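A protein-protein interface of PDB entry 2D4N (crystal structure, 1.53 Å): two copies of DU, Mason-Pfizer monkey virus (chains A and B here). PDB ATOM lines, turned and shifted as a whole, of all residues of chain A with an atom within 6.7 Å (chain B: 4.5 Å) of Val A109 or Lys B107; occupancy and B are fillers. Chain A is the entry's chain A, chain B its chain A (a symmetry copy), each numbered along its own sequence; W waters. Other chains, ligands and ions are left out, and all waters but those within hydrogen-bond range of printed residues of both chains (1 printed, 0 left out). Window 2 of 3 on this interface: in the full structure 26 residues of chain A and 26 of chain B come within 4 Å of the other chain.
Printed residues of chain B within 4 Å of Val A109: Tyr B90 and Lys B107. Of the printed residues of chain A, Lys B107 touches Val A109. Of the printed residues of chain A, Gly B56 touches Asn A110 (3.5 Å). Of the printed residues of chain B, Thr A83 touches Pro B57 (3.5 Å) and Tyr B90 (3.6 Å). The nearest printed residue of chain B that does not touch Val A109 is Pro B57 (4.3 Å). The nearest printed residue of chain A that does not touch Lys B107 is Asn A110 (4.03 Å). The nearest printed residue of chain A that does not touch Gln B88 is Val A109 (6.6 Å).
The side-chain amide oxygen (OE1) of Gln A88 lies close to the side-chain amide oxygen (OE1) of Gln B88, 3.0 Å away. O of Pro B53 sits close to OD1 of Asn A110.
The backbone carbonyl oxygen (O) of Gly A86 sits at hydrogen-bond distance from the backbone NH (N) of Val A109 (2.8 Å). The backbone carbonyl oxygen (O) of Gln A88 sits at hydrogen-bond distance from the backbone NH (N) of Lys A107. NZ of Lys A107 sits at hydrogen-bond distance from O of Val A109, 3.2 Å away. The backbone NH (N) of Lys B107 sits at hydrogen-bond distance from the backbone carbonyl oxygen (O) of Gln B88, at 2.8 Å. The side-chain amino group of Lys B107 is in hydrogen-bond range of the backbone carbonyl oxygen of Val B109, 3.2 Å away.
Water W1 lies within hydrogen-bond range of OH of Tyr B90 (2.6 Å), NE2 of Gln B88 (2.9 Å) and NE2 of Gln A88 (3.1 Å).
Among the printed residues, pairs that only touch across the chains: Asn A110 with Gly B56 (3.5 Å), Thr A83 with Pro B57 (3.5 Å), Thr A83 with Tyr B90 (3.6 Å), Val A109 with Lys B107 (3.7 Å), Val A109 with Tyr B90 (3.8 Å) and Gln A88 with Tyr B90 (3.8 Å).
Gln B88 touches its own counterpart, Gln A88. Val A109 touches Lys B107, but with the chains exchanged Lys A107 does not touch Val B109 (8.7 Å). Positions printed for both chains: 53, 86, 87, 88, 107, 108 and 109.
Of the 12 printed residues of chain A, 4 touch a printed residue of chain B. Hydrophobic or aromatic side chains of chain A within 4 Å of the printed part of chain B: Val A109. Among the printed residues, 8 pairs touch across the chains. Among the printed residues, no Asp or Glu carboxylate lies within 4 Å of a Lys or Arg side-chain nitrogen of the other chain.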
ATOM      1  N   THR A  52      34.764   6.655 -22.719  1.00  0.00           N
ATOM      2  CA  THR A  52      35.051   6.816 -21.294  1.00  0.00           C
ATOM      3  C   THR A  52      33.864   7.497 -20.656  1.00  0.00           C
ATOM      4  O   THR A  52      33.087   8.147 -21.340  1.00  0.00           O
ATOM      5  CB  THR A  52      36.253   7.698 -21.032  1.00  0.00           C
ATOM      6  OG1 THR A  52      36.008   8.977 -21.633  1.00  0.00           O
ATOM      7  CG2 THR A  52      37.505   7.023 -21.624  1.00  0.00           C
ATOM      8  N   PRO A  53      33.680   7.289 -19.342  1.00  0.00           N
ATOM      9  CA  PRO A  53      32.473   7.933 -18.753  1.00  0.00           C
ATOM     10  C   PRO A  53      32.416   9.462 -18.943  1.00  0.00           C
ATOM     11  O   PRO A  53      31.315  10.017 -19.246  1.00  0.00           O
ATOM     12  CB  PRO A  53      32.536   7.544 -17.282  1.00  0.00           C
ATOM     13  CG  PRO A  53      33.366   6.330 -17.228  1.00  0.00           C
ATOM     14  CD  PRO A  53      34.356   6.381 -18.415  1.00  0.00           C
ATOM     15  N   THR A  83      25.102  -4.187 -22.447  1.00  0.00           N
ATOM     16  CA  THR A  83      24.718  -3.420 -21.265  1.00  0.00           C
ATOM     17  C   THR A  83      25.487  -3.917 -20.024  1.00  0.00           C
ATOM     18  O   THR A  83      26.075  -3.126 -19.271  1.00  0.00           O
ATOM     19  CB  THR A  83      23.206  -3.567 -21.043  1.00  0.00           C
ATOM     20  OG1 THR A  83      22.482  -3.101 -22.199  1.00  0.00           O
ATOM     21  CG2 THR A  83      22.765  -2.812 -19.759  1.00  0.00           C
ATOM     22  N   GLY A  86      28.950  -2.723 -19.479  1.00  0.00           N
ATOM     23  CA  GLY A  86      29.087  -1.315 -19.084  1.00  0.00           C
ATOM     24  C   GLY A  86      28.910  -0.294 -20.196  1.00  0.00           C
ATOM     25  O   GLY A  86      29.240   0.881 -20.004  1.00  0.00           O
ATOM     26  N   LEU A  87      28.369  -0.706 -21.347  1.00  0.00           N
ATOM     27  CA  LEU A  87      28.050   0.251 -22.392  1.00  0.00           C
ATOM     28  C   LEU A  87      26.534   0.394 -22.435  1.00  0.00           C
ATOM     29  O   LEU A  87      25.815  -0.568 -22.784  1.00  0.00           O
ATOM     30  CB  LEU A  87      28.535  -0.248 -23.754  1.00  0.00           C
ATOM     31  CG  LEU A  87      28.283   0.718 -24.928  1.00  0.00           C
ATOM     32  CD1 LEU A  87      29.153   1.943 -24.743  1.00  0.00           C
ATOM     33  CD2 LEU A  87      28.700  -0.029 -26.163  1.00  0.00           C
ATOM     34  N   GLN A  88      26.082   1.553 -22.046  1.00  0.00           N
ATOM     35  CA  GLN A  88      24.664   1.881 -22.035  1.00  0.00           C
ATOM     36  C   GLN A  88      24.249   2.407 -23.402  1.00  0.00           C
ATOM     37  O   GLN A  88      24.850   3.367 -23.947  1.00  0.00           O
ATOM     38  CB  GLN A  88      24.379   2.969 -20.983  1.00  0.00           C
ATOM     39  CG  GLN A  88      22.937   3.502 -21.090  1.00  0.00           C
ATOM     40  CD  GLN A  88      22.520   4.378 -19.925  1.00  0.00           C
ATOM     41  OE1 GLN A  88      21.323   4.554 -19.683  1.00  0.00           O
ATOM     42  NE2 GLN A  88      23.488   4.979 -19.238  1.00  0.00           N
ATOM     43  N   LYS A 107      26.830   5.399 -24.097  1.00  0.00           N
ATOM     44  CA  LYS A 107      27.739   5.987 -23.097  1.00  0.00           C
ATOM     45  C   LYS A 107      28.379   4.866 -22.266  1.00  0.00           C
ATOM     46  O   LYS A 107      27.764   3.875 -21.875  1.00  0.00           O
ATOM     47  CB  LYS A 107      27.030   7.038 -22.190  1.00  0.00           C
ATOM     48  CG  LYS A 107      27.949   7.554 -21.054  1.00  0.00           C
ATOM     49  CD  LYS A 107      27.192   8.264 -19.943  1.00  0.00           C
ATOM     50  CE  LYS A 107      28.151   8.772 -18.877  1.00  0.00           C
ATOM     51  NZ  LYS A 107      28.513   7.763 -17.856  1.00  0.00           N
ATOM     52  N   ALA A 108      29.683   5.043 -21.991  1.00  0.00           N
ATOM     53  CA  ALA A 108      30.376   4.192 -21.048  1.00  0.00           C
ATOM     54  C   ALA A 108      29.895   4.532 -19.626  1.00  0.00           C
ATOM     55  O   ALA A 108      29.932   5.672 -19.190  1.00  0.00           O
ATOM     56  CB  ALA A 108      31.939   4.321 -21.154  1.00  0.00           C
ATOM     57  N   VAL A 109      29.435   3.503 -18.908  1.00  0.00           N
ATOM     58  CA  VAL A 109      28.716   3.772 -17.642  1.00  0.00           C
ATOM     59  C   VAL A 109      29.641   4.242 -16.509  1.00  0.00           C
ATOM     60  O   VAL A 109      29.476   5.347 -15.933  1.00  0.00           O
ATOM     61  CB  VAL A 109      27.898   2.544 -17.226  1.00  0.00           C
ATOM     62  CG1 VAL A 109      27.515   2.610 -15.793  1.00  0.00           C
ATOM     63  CG2 VAL A 109      26.651   2.467 -18.127  1.00  0.00           C
ATOM     64  N   ASN A 110      30.614   3.424 -16.185  1.00  0.00           N
ATOM     65  CA  ASN A 110      31.550   3.903 -15.190  1.00  0.00           C
ATOM     66  C   ASN A 110      32.989   3.381 -15.369  1.00  0.00           C
ATOM     67  O   ASN A 110      33.877   3.755 -14.585  1.00  0.00           O
ATOM     68  CB  ASN A 110      30.983   3.814 -13.739  1.00  0.00           C
ATOM     69  CG  ASN A 110      30.706   2.415 -13.321  1.00  0.00           C
ATOM     70  OD1 ASN A 110      30.028   2.175 -12.333  1.00  0.00           O
ATOM     71  ND2 ASN A 110      31.213   1.469 -14.089  1.00  0.00           N
ATOM     72  N   ASN A 111      33.225   2.563 -16.403  1.00  0.00           N
ATOM     73  CA  ASN A 111      34.570   2.165 -16.810  1.00  0.00           C
ATOM     74  C   ASN A 111      34.820   2.512 -18.266  1.00  0.00           C
ATOM     75  O   ASN A 111      33.878   2.864 -18.968  1.00  0.00           O
ATOM     76  CB  ASN A 111      34.786   0.655 -16.669  1.00  0.00           C
ATOM     77  CG  ASN A 111      34.587   0.167 -15.249  1.00  0.00           C
ATOM     78  OD1 ASN A 111      35.206   0.673 -14.313  1.00  0.00           O
ATOM     79  ND2 ASN A 111      33.732  -0.835 -15.084  1.00  0.00           N
ATOM     80  N   VAL A 113      35.162   1.616 -22.000  1.00  0.00           N
ATOM     81  CA  VAL A 113      34.634   0.581 -22.911  1.00  0.00           C
ATOM     82  C   VAL A 113      35.237   0.677 -24.294  1.00  0.00           C
ATOM     83  O   VAL A 113      35.369   1.779 -24.840  1.00  0.00           O
ATOM     84  CB  VAL A 113      33.087   0.787 -23.060  1.00  0.00           C
ATOM     85  CG1 VAL A 113      32.541  -0.131 -24.156  1.00  0.00           C
ATOM     86  CG2 VAL A 113      32.420   0.529 -21.741  1.00  0.00           C
ATOM     87  N   PRO B  53      26.748   2.947  -6.711  1.00  0.00           N
ATOM     88  CA  PRO B  53      27.048   3.381  -8.104  1.00  0.00           C
ATOM     89  C   PRO B  53      28.311   2.734  -8.708  1.00  0.00           C
ATOM     90  O   PRO B  53      28.298   2.341  -9.915  1.00  0.00           O
ATOM     91  CB  PRO B  53      27.182   4.894  -7.992  1.00  0.00           C
ATOM     92  CG  PRO B  53      26.439   5.269  -6.778  1.00  0.00           C
ATOM     93  CD  PRO B  53      26.485   4.068  -5.807  1.00  0.00           C
ATOM     94  N   GLY B  56      28.299  -0.539 -10.950  1.00  0.00           N
ATOM     95  CA  GLY B  56      27.776  -0.682 -12.346  1.00  0.00           C
ATOM     96  C   GLY B  56      26.620  -1.708 -12.496  1.00  0.00           C
ATOM     97  O   GLY B  56      25.974  -2.104 -11.504  1.00  0.00           O
ATOM     98  N   PRO B  57      26.303  -2.084 -13.740  1.00  0.00           N
ATOM     99  CA  PRO B  57      25.138  -2.926 -13.999  1.00  0.00           C
ATOM    100  C   PRO B  57      25.187  -4.283 -13.295  1.00  0.00           C
ATOM    101  O   PRO B  57      26.202  -4.971 -13.341  1.00  0.00           O
ATOM    102  CB  PRO B  57      25.218  -3.155 -15.509  1.00  0.00           C
ATOM    103  CG  PRO B  57      25.845  -1.828 -15.991  1.00  0.00           C
ATOM    104  CD  PRO B  57      26.946  -1.616 -14.982  1.00  0.00           C
ATOM    105  N   GLY B  86      16.177   6.176  -7.401  1.00  0.00           N
ATOM    106  CA  GLY B  86      17.585   6.110  -7.818  1.00  0.00           C
ATOM    107  C   GLY B  86      18.073   4.751  -8.289  1.00  0.00           C
ATOM    108  O   GLY B  86      19.285   4.552  -8.428  1.00  0.00           O
ATOM    109  N   LEU B  87      17.159   3.817  -8.569  1.00  0.00           N
ATOM    110  CA  LEU B  87      17.561   2.549  -9.153  1.00  0.00           C
ATOM    111  C   LEU B  87      17.114   2.554 -10.610  1.00  0.00           C
ATOM    112  O   LEU B  87      15.898   2.561 -10.901  1.00  0.00           O
ATOM    113  CB  LEU B  87      16.884   1.380  -8.436  1.00  0.00           C
ATOM    114  CG  LEU B  87      17.278  -0.017  -8.955  1.00  0.00           C
ATOM    115  CD1 LEU B  87      18.729  -0.270  -8.609  1.00  0.00           C
ATOM    116  CD2 LEU B  87      16.397  -0.985  -8.216  1.00  0.00           C
ATOM    117  N   GLN B  88      18.084   2.593 -11.480  1.00  0.00           N
ATOM    118  CA  GLN B  88      17.852   2.588 -12.917  1.00  0.00           C
ATOM    119  C   GLN B  88      17.741   1.152 -13.411  1.00  0.00           C
ATOM    120  O   GLN B  88      18.637   0.304 -13.175  1.00  0.00           O
ATOM    121  CB  GLN B  88      19.024   3.270 -13.647  1.00  0.00           C
ATOM    122  CG  GLN B  88      18.927   3.090 -15.174  1.00  0.00           C
ATOM    123  CD  GLN B  88      19.899   3.952 -15.955  1.00  0.00           C
ATOM    124  OE1 GLN B  88      19.687   4.197 -17.145  1.00  0.00           O
ATOM    125  NE2 GLN B  88      20.995   4.362 -15.320  1.00  0.00           N
ATOM    126  N   TYR B  90      17.811  -0.907 -16.898  1.00  0.00           N
ATOM    127  CA  TYR B  90      18.137  -0.673 -18.271  1.00  0.00           C
ATOM    128  C   TYR B  90      17.125  -1.466 -19.083  1.00  0.00           C
ATOM    129  O   TYR B  90      16.888  -2.680 -18.832  1.00  0.00           O
ATOM    130  CB  TYR B  90      19.495  -1.276 -18.603  1.00  0.00           C
ATOM    131  CG  TYR B  90      20.612  -0.563 -17.909  1.00  0.00           C
ATOM    132  CD1 TYR B  90      20.938   0.744 -18.269  1.00  0.00           C
ATOM    133  CD2 TYR B  90      21.284  -1.181 -16.821  1.00  0.00           C
ATOM    134  CE1 TYR B  90      21.992   1.437 -17.589  1.00  0.00           C
ATOM    135  CE2 TYR B  90      22.381  -0.527 -16.159  1.00  0.00           C
ATOM    136  CZ  TYR B  90      22.702   0.798 -16.552  1.00  0.00           C
ATOM    137  OH  TYR B  90      23.765   1.479 -15.920  1.00  0.00           O
ATOM    138  N   ALA B 106      20.155  -3.767 -13.625  1.00  0.00           N
ATOM    139  CA  ALA B 106      19.898  -2.569 -12.795  1.00  0.00           C
ATOM    140  C   ALA B 106      21.198  -1.878 -12.359  1.00  0.00           C
ATOM    141  O   ALA B 106      22.202  -2.526 -12.178  1.00  0.00           O
ATOM    142  CB  ALA B 106      19.163  -2.991 -11.555  1.00  0.00           C
ATOM    143  N   LYS B 107      21.104  -0.581 -12.077  1.00  0.00           N
ATOM    144  CA  LYS B 107      22.262   0.134 -11.512  1.00  0.00           C
ATOM    145  C   LYS B 107      21.770   1.230 -10.557  1.00  0.00           C
ATOM    146  O   LYS B 107      20.793   1.942 -10.786  1.00  0.00           O
ATOM    147  CB  LYS B 107      23.201   0.714 -12.612  1.00  0.00           C
ATOM    148  CG  LYS B 107      24.341   1.581 -12.020  1.00  0.00           C
ATOM    149  CD  LYS B 107      25.026   2.462 -13.052  1.00  0.00           C
ATOM    150  CE  LYS B 107      26.152   3.261 -12.415  1.00  0.00           C
ATOM    151  NZ  LYS B 107      25.715   4.520 -11.770  1.00  0.00           N
ATOM    152  N   ALA B 108      22.491   1.359  -9.428  1.00  0.00           N
ATOM    153  CA  ALA B 108      22.289   2.475  -8.530  1.00  0.00           C
ATOM    154  C   ALA B 108      22.846   3.750  -9.189  1.00  0.00           C
ATOM    155  O   ALA B 108      23.994   3.812  -9.602  1.00  0.00           O
ATOM    156  CB  ALA B 108      22.945   2.243  -7.122  1.00  0.00           C
ATOM    157  N   VAL B 109      21.994   4.776  -9.281  1.00  0.00           N
ATOM    158  CA  VAL B 109      22.354   5.937 -10.124  1.00  0.00           C
ATOM    159  C   VAL B 109      23.455   6.815  -9.509  1.00  0.00           C
ATOM    160  O   VAL B 109      24.541   7.032 -10.104  1.00  0.00           O
ATOM    161  CB  VAL B 109      21.103   6.759 -10.456  1.00  0.00           C
ATOM    162  CG1 VAL B 109      21.459   8.123 -10.923  1.00  0.00           C
ATOM    163  CG2 VAL B 109      20.298   6.002 -11.529  1.00  0.00           C
HETATM  164  O   HOH W   1      23.691   4.029 -16.328  1.00  0.00           O
